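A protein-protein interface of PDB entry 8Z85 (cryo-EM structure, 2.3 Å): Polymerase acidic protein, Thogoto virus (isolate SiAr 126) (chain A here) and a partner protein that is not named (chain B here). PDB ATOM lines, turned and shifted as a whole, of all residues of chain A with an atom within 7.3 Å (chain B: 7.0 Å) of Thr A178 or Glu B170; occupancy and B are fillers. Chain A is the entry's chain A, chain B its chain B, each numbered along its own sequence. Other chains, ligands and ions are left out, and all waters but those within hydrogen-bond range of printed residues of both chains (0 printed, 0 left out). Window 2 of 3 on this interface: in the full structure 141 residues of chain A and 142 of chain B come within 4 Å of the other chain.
The side-chain hydroxyl of Thr A178 is in hydrogen-bond range of the side-chain carboxylate of Glu B170 (3.1 Å). The backbone NH of Phe A179 lies within hydrogen-bond range of the side-chain carboxylate of Glu B170, at 2.7 Å.
The side-chain hydroxyl (OG1) of Thr A181 lies close to the backbone carbonyl oxygen (O) of Thr A177, at 3.5 Å. OG1 of Thr A181 sits at hydrogen-bond distance from O of Thr A178 (2.5 Å). The guanidinium group (NH1) of Arg B216 sits at hydrogen-bond distance from the backbone carbonyl oxygen (O) of Leu B171. The side-chain carboxylate (OD1) of Asp B172 is in salt-bridge range of the guanidinium group (NH1) of Arg B216.
Ala B166 touches Ser A174. Gly A176 touches Glu B170 (CA to OE2, 3.1 Å). Thr A177 touches Glu B170. Thr A178 touches Arg B216. Ala B166 touches Phe A179. Met B169 touches Phe A179 (CB to CD1, 3.99 Å). Arg B216 touches Leu A182.
Thr A178 touches just these residues of chain B: Glu B170 and Arg B216. Ala B164 touches none of the printed residues of chain A. Printed residues of chain A within 4 Å of Ala B166: Ser A174 and Phe A179. Of the printed residues of chain A, Met B169 touches Phe A179. Glu B170 touches four residues of chain A. Leu B171 touches none of the printed residues of chain A. Of the printed residues of chain A, Arg B216 touches Thr A178 (3.4 Å) and Leu A182 (3.98 Å). The nearest residue of chain A that does not touch Glu B170 is Arg A180 (4.7 Å). The nearest printed residue of chain B that does not touch Ser A174 is Asp B167 (5.1 Å).
Of the 11 printed residues of chain A, 6 touch a printed residue of chain B. Printed residues of chain A that touch a printed residue of chain B: Ser A174, Gly A176, Thr A177, Thr A178, Phe A179 and Leu A182. Along chain A the printed residues that touch a printed residue of chain B span positions 174 to 182. Of the 11 printed residues of chain B, 4 touch a printed residue of chain A. Printed residues of chain B that touch a printed residue of chain A: Ala B166, Met B169, Glu B170 and Arg B216. Among the printed residues, no Asp or Glu carboxylate lies within 4 Å of a Lys or Arg side-chain nitrogen of the other chain.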
ATOM      1  N   SER A 174     -27.399  30.602   6.872  1.00  0.00           N
ATOM      2  CA  SER A 174     -28.656  30.038   6.408  1.00  0.00           C
ATOM      3  C   SER A 174     -28.570  29.792   4.910  1.00  0.00           C
ATOM      4  O   SER A 174     -27.846  30.484   4.192  1.00  0.00           O
ATOM      5  CB  SER A 174     -29.841  30.960   6.725  1.00  0.00           C
ATOM      6  OG  SER A 174     -29.573  32.291   6.323  1.00  0.00           O
ATOM      7  N   VAL A 175     -29.318  28.794   4.446  1.00  0.00           N
ATOM      8  CA  VAL A 175     -29.371  28.427   3.037  1.00  0.00           C
ATOM      9  C   VAL A 175     -30.784  28.678   2.534  1.00  0.00           C
ATOM     10  O   VAL A 175     -31.754  28.162   3.102  1.00  0.00           O
ATOM     11  CB  VAL A 175     -28.961  26.961   2.817  1.00  0.00           C
ATOM     12  CG1 VAL A 175     -28.702  26.697   1.343  1.00  0.00           C
ATOM     13  CG2 VAL A 175     -27.735  26.623   3.647  1.00  0.00           C
ATOM     14  N   GLY A 176     -30.900  29.467   1.468  1.00  0.00           N
ATOM     15  CA  GLY A 176     -32.199  29.792   0.921  1.00  0.00           C
ATOM     16  C   GLY A 176     -32.809  28.652   0.131  1.00  0.00           C
ATOM     17  O   GLY A 176     -32.197  27.610  -0.095  1.00  0.00           O
ATOM     18  N   THR A 177     -34.057  28.869  -0.291  1.00  0.00           N
ATOM     19  CA  THR A 177     -34.784  27.837  -1.025  1.00  0.00           C
ATOM     20  C   THR A 177     -34.141  27.550  -2.377  1.00  0.00           C
ATOM     21  O   THR A 177     -33.997  26.384  -2.766  1.00  0.00           O
ATOM     22  CB  THR A 177     -36.243  28.255  -1.206  1.00  0.00           C
ATOM     23  OG1 THR A 177     -36.851  28.441   0.078  1.00  0.00           O
ATOM     24  CG2 THR A 177     -37.014  27.192  -1.975  1.00  0.00           C
ATOM     25  N   THR A 178     -33.747  28.596  -3.106  1.00  0.00           N
ATOM     26  CA  THR A 178     -33.207  28.398  -4.448  1.00  0.00           C
ATOM     27  C   THR A 178     -31.852  27.701  -4.409  1.00  0.00           C
ATOM     28  O   THR A 178     -31.597  26.787  -5.201  1.00  0.00           O
ATOM     29  CB  THR A 178     -33.100  29.735  -5.178  1.00  0.00           C
ATOM     30  OG1 THR A 178     -34.318  30.471  -5.008  1.00  0.00           O
ATOM     31  CG2 THR A 178     -32.861  29.508  -6.659  1.00  0.00           C
ATOM     32  N   PHE A 179     -30.970  28.121  -3.500  1.00  0.00           N
ATOM     33  CA  PHE A 179     -29.676  27.459  -3.370  1.00  0.00           C
ATOM     34  C   PHE A 179     -29.832  26.019  -2.899  1.00  0.00           C
ATOM     35  O   PHE A 179     -29.038  25.153  -3.285  1.00  0.00           O
ATOM     36  CB  PHE A 179     -28.780  28.237  -2.406  1.00  0.00           C
ATOM     37  CG  PHE A 179     -27.330  27.851  -2.479  1.00  0.00           C
ATOM     38  CD1 PHE A 179     -26.791  27.341  -3.649  1.00  0.00           C
ATOM     39  CD2 PHE A 179     -26.506  27.993  -1.376  1.00  0.00           C
ATOM     40  CE1 PHE A 179     -25.458  26.985  -3.716  1.00  0.00           C
ATOM     41  CE2 PHE A 179     -25.173  27.640  -1.438  1.00  0.00           C
ATOM     42  CZ  PHE A 179     -24.649  27.134  -2.609  1.00  0.00           C
ATOM     43  N   ARG A 180     -30.839  25.748  -2.067  1.00  0.00           N
ATOM     44  CA  ARG A 180     -31.063  24.389  -1.590  1.00  0.00           C
ATOM     45  C   ARG A 180     -31.436  23.454  -2.733  1.00  0.00           C
ATOM     46  O   ARG A 180     -30.983  22.304  -2.778  1.00  0.00           O
ATOM     47  CB  ARG A 180     -32.151  24.392  -0.516  1.00  0.00           C
ATOM     48  CG  ARG A 180     -32.257  23.102   0.272  1.00  0.00           C
ATOM     49  CD  ARG A 180     -33.261  23.241   1.402  1.00  0.00           C
ATOM     50  NE  ARG A 180     -32.849  24.249   2.371  1.00  0.00           N
ATOM     51  CZ  ARG A 180     -32.177  23.990   3.483  1.00  0.00           C
ATOM     52  NH1 ARG A 180     -31.822  22.757   3.804  1.00  0.00           N
ATOM     53  NH2 ARG A 180     -31.850  24.993   4.294  1.00  0.00           N
ATOM     54  N   THR A 181     -32.269  23.926  -3.664  1.00  0.00           N
ATOM     55  CA  THR A 181     -32.672  23.091  -4.793  1.00  0.00           C
ATOM     56  C   THR A 181     -31.488  22.760  -5.692  1.00  0.00           C
ATOM     57  O   THR A 181     -31.373  21.630  -6.183  1.00  0.00           O
ATOM     58  CB  THR A 181     -33.772  23.786  -5.594  1.00  0.00           C
ATOM     59  OG1 THR A 181     -33.354  25.115  -5.932  1.00  0.00           O
ATOM     60  CG2 THR A 181     -35.056  23.858  -4.783  1.00  0.00           C
ATOM     61  N   LEU A 182     -30.606  23.732  -5.931  1.00  0.00           N
ATOM     62  CA  LEU A 182     -29.438  23.486  -6.772  1.00  0.00           C
ATOM     63  C   LEU A 182     -28.515  22.449  -6.147  1.00  0.00           C
ATOM     64  O   LEU A 182     -27.971  21.586  -6.848  1.00  0.00           O
ATOM     65  CB  LEU A 182     -28.679  24.792  -7.017  1.00  0.00           C
ATOM     66  CG  LEU A 182     -29.061  25.678  -8.206  1.00  0.00           C
ATOM     67  CD1 LEU A 182     -30.568  25.821  -8.355  1.00  0.00           C
ATOM     68  CD2 LEU A 182     -28.405  27.044  -8.076  1.00  0.00           C
ATOM     69  N   LEU A 183     -28.324  22.517  -4.829  1.00  0.00           N
ATOM     70  CA  LEU A 183     -27.394  21.625  -4.147  1.00  0.00           C
ATOM     71  C   LEU A 183     -27.852  20.172  -4.159  1.00  0.00           C
ATOM     72  O   LEU A 183     -27.022  19.276  -3.972  1.00  0.00           O
ATOM     73  CB  LEU A 183     -27.195  22.089  -2.704  1.00  0.00           C
ATOM     74  CG  LEU A 183     -26.301  23.312  -2.499  1.00  0.00           C
ATOM     75  CD1 LEU A 183     -26.480  23.878  -1.102  1.00  0.00           C
ATOM     76  CD2 LEU A 183     -24.848  22.957  -2.750  1.00  0.00           C
ATOM     77  N   ARG A 185     -29.350  18.465  -6.700  1.00  0.00           N
ATOM     78  CA  ARG A 185     -29.582  17.891  -8.022  1.00  0.00           C
ATOM     79  C   ARG A 185     -28.790  16.607  -8.242  1.00  0.00           C
ATOM     80  O   ARG A 185     -29.255  15.716  -8.962  1.00  0.00           O
ATOM     81  CB  ARG A 185     -29.237  18.908  -9.110  1.00  0.00           C
ATOM     82  CG  ARG A 185     -30.196  20.081  -9.197  1.00  0.00           C
ATOM     83  CD  ARG A 185     -29.696  21.116 -10.189  1.00  0.00           C
ATOM     84  NE  ARG A 185     -30.636  22.220 -10.349  1.00  0.00           N
ATOM     85  CZ  ARG A 185     -30.416  23.285 -11.105  1.00  0.00           C
ATOM     86  NH1 ARG A 185     -29.290  23.431 -11.784  1.00  0.00           N
ATOM     87  NH2 ARG A 185     -31.351  24.228 -11.187  1.00  0.00           N
ATOM     88  N   ALA B 164     -22.338  35.306   2.276  1.00  0.00           N
ATOM     89  CA  ALA B 164     -22.497  36.047   1.028  1.00  0.00           C
ATOM     90  C   ALA B 164     -22.602  35.106  -0.164  1.00  0.00           C
ATOM     91  O   ALA B 164     -23.381  35.353  -1.092  1.00  0.00           O
ATOM     92  CB  ALA B 164     -21.332  37.017   0.844  1.00  0.00           C
ATOM     93  N   ILE B 165     -21.817  34.026  -0.162  1.00  0.00           N
ATOM     94  CA  ILE B 165     -21.892  33.046  -1.243  1.00  0.00           C
ATOM     95  C   ILE B 165     -23.278  32.421  -1.300  1.00  0.00           C
ATOM     96  O   ILE B 165     -23.848  32.233  -2.381  1.00  0.00           O
ATOM     97  CB  ILE B 165     -20.795  31.978  -1.075  1.00  0.00           C
ATOM     98  CG1 ILE B 165     -19.409  32.624  -1.094  1.00  0.00           C
ATOM     99  CG2 ILE B 165     -20.903  30.925  -2.164  1.00  0.00           C
ATOM    100  CD1 ILE B 165     -19.087  33.332  -2.388  1.00  0.00           C
ATOM    101  N   ALA B 166     -23.844  32.085  -0.139  1.00  0.00           N
ATOM    102  CA  ALA B 166     -25.194  31.533  -0.115  1.00  0.00           C
ATOM    103  C   ALA B 166     -26.230  32.559  -0.555  1.00  0.00           C
ATOM    104  O   ALA B 166     -27.223  32.197  -1.195  1.00  0.00           O
ATOM    105  CB  ALA B 166     -25.524  31.011   1.282  1.00  0.00           C
ATOM    106  N   ASP B 167     -26.020  33.834  -0.223  1.00  0.00           N
ATOM    107  CA  ASP B 167     -26.993  34.864  -0.569  1.00  0.00           C
ATOM    108  C   ASP B 167     -26.945  35.224  -2.050  1.00  0.00           C
ATOM    109  O   ASP B 167     -27.988  35.489  -2.657  1.00  0.00           O
ATOM    110  CB  ASP B 167     -26.761  36.111   0.285  1.00  0.00           C
ATOM    111  CG  ASP B 167     -27.107  35.891   1.743  1.00  0.00           C
ATOM    112  OD1 ASP B 167     -27.992  35.056   2.027  1.00  0.00           O
ATOM    113  OD2 ASP B 167     -26.495  36.553   2.607  1.00  0.00           O
ATOM    114  N   VAL B 168     -25.749  35.248  -2.645  1.00  0.00           N
ATOM    115  CA  VAL B 168     -25.629  35.691  -4.032  1.00  0.00           C
ATOM    116  C   VAL B 168     -26.308  34.709  -4.982  1.00  0.00           C
ATOM    117  O   VAL B 168     -26.864  35.116  -6.008  1.00  0.00           O
ATOM    118  CB  VAL B 168     -24.149  35.921  -4.402  1.00  0.00           C
ATOM    119  CG1 VAL B 168     -23.364  34.621  -4.378  1.00  0.00           C
ATOM    120  CG2 VAL B 168     -24.036  36.598  -5.759  1.00  0.00           C
ATOM    121  N   MET B 169     -26.285  33.412  -4.665  1.00  0.00           N
ATOM    122  CA  MET B 169     -26.964  32.435  -5.507  1.00  0.00           C
ATOM    123  C   MET B 169     -28.480  32.524  -5.415  1.00  0.00           C
ATOM    124  O   MET B 169     -29.167  31.941  -6.260  1.00  0.00           O
ATOM    125  CB  MET B 169     -26.504  31.021  -5.156  1.00  0.00           C
ATOM    126  CG  MET B 169     -25.003  30.894  -5.013  1.00  0.00           C
ATOM    127  SD  MET B 169     -24.213  30.746  -6.626  1.00  0.00           S
ATOM    128  CE  MET B 169     -25.334  29.616  -7.446  1.00  0.00           C
ATOM    129  N   GLU B 170     -29.016  33.226  -4.418  1.00  0.00           N
ATOM    130  CA  GLU B 170     -30.450  33.480  -4.376  1.00  0.00           C
ATOM    131  C   GLU B 170     -30.872  34.565  -5.355  1.00  0.00           C
ATOM    132  O   GLU B 170     -32.057  34.648  -5.695  1.00  0.00           O
ATOM    133  CB  GLU B 170     -30.876  33.860  -2.958  1.00  0.00           C
ATOM    134  CG  GLU B 170     -30.712  32.730  -1.962  1.00  0.00           C
ATOM    135  CD  GLU B 170     -31.656  31.580  -2.240  1.00  0.00           C
ATOM    136  OE1 GLU B 170     -32.787  31.836  -2.703  1.00  0.00           O
ATOM    137  OE2 GLU B 170     -31.260  30.417  -2.016  1.00  0.00           O
ATOM    138  N   LEU B 171     -29.934  35.389  -5.814  1.00  0.00           N
ATOM    139  CA  LEU B 171     -30.251  36.424  -6.784  1.00  0.00           C
ATOM    140  C   LEU B 171     -30.527  35.806  -8.149  1.00  0.00           C
ATOM    141  O   LEU B 171     -29.865  34.850  -8.561  1.00  0.00           O
ATOM    142  CB  LEU B 171     -29.102  37.425  -6.887  1.00  0.00           C
ATOM    143  CG  LEU B 171     -28.762  38.219  -5.626  1.00  0.00           C
ATOM    144  CD1 LEU B 171     -27.910  39.427  -5.975  1.00  0.00           C
ATOM    145  CD2 LEU B 171     -30.029  38.649  -4.906  1.00  0.00           C
ATOM    146  N   ASP B 172     -31.516  36.360  -8.852  1.00  0.00           N
ATOM    147  CA  ASP B 172     -31.821  35.875 -10.193  1.00  0.00           C
ATOM    148  C   ASP B 172     -30.688  36.176 -11.164  1.00  0.00           C
ATOM    149  O   ASP B 172     -30.358  35.342 -12.015  1.00  0.00           O
ATOM    150  CB  ASP B 172     -33.129  36.486 -10.695  1.00  0.00           C
ATOM    151  CG  ASP B 172     -34.337  35.638 -10.351  1.00  0.00           C
ATOM    152  OD1 ASP B 172     -34.153  34.450 -10.019  1.00  0.00           O
ATOM    153  OD2 ASP B 172     -35.471  36.158 -10.418  1.00  0.00           O
ATOM    154  N   GLU B 173     -30.082  37.356 -11.061  1.00  0.00           N
ATOM    155  CA  GLU B 173     -29.107  37.784 -12.049  1.00  0.00           C
ATOM    156  C   GLU B 173     -27.974  38.509 -11.332  1.00  0.00           C
ATOM    157  O   GLU B 173     -28.200  39.197 -10.333  1.00  0.00           O
ATOM    158  CB  GLU B 173     -29.774  38.693 -13.092  1.00  0.00           C
ATOM    159  CG  GLU B 173     -28.884  39.152 -14.217  1.00  0.00           C
ATOM    160  CD  GLU B 173     -28.446  37.985 -15.082  1.00  0.00           C
ATOM    161  OE1 GLU B 173     -29.176  36.972 -15.127  1.00  0.00           O
ATOM    162  OE2 GLU B 173     -27.389  38.076 -15.726  1.00  0.00           O
ATOM    163  N   ARG B 216     -28.154  32.786 -12.842  1.00  0.00           N
ATOM    164  CA  ARG B 216     -28.018  31.865 -11.719  1.00  0.00           C
ATOM    165  C   ARG B 216     -27.350  30.565 -12.148  1.00  0.00           C
ATOM    166  O   ARG B 216     -26.471  30.054 -11.446  1.00  0.00           O
ATOM    167  CB  ARG B 216     -29.379  31.575 -11.088  1.00  0.00           C
ATOM    168  CG  ARG B 216     -29.269  30.768  -9.802  1.00  0.00           C
ATOM    169  CD  ARG B 216     -30.578  30.100  -9.415  1.00  0.00           C
ATOM    170  NE  ARG B 216     -31.740  30.727 -10.035  1.00  0.00           N
ATOM    171  CZ  ARG B 216     -32.404  31.751  -9.518  1.00  0.00           C
ATOM    172  NH1 ARG B 216     -32.044  32.300  -8.370  1.00  0.00           N
ATOM    173  NH2 ARG B 216     -33.457  32.235 -10.169  1.00  0.00           N
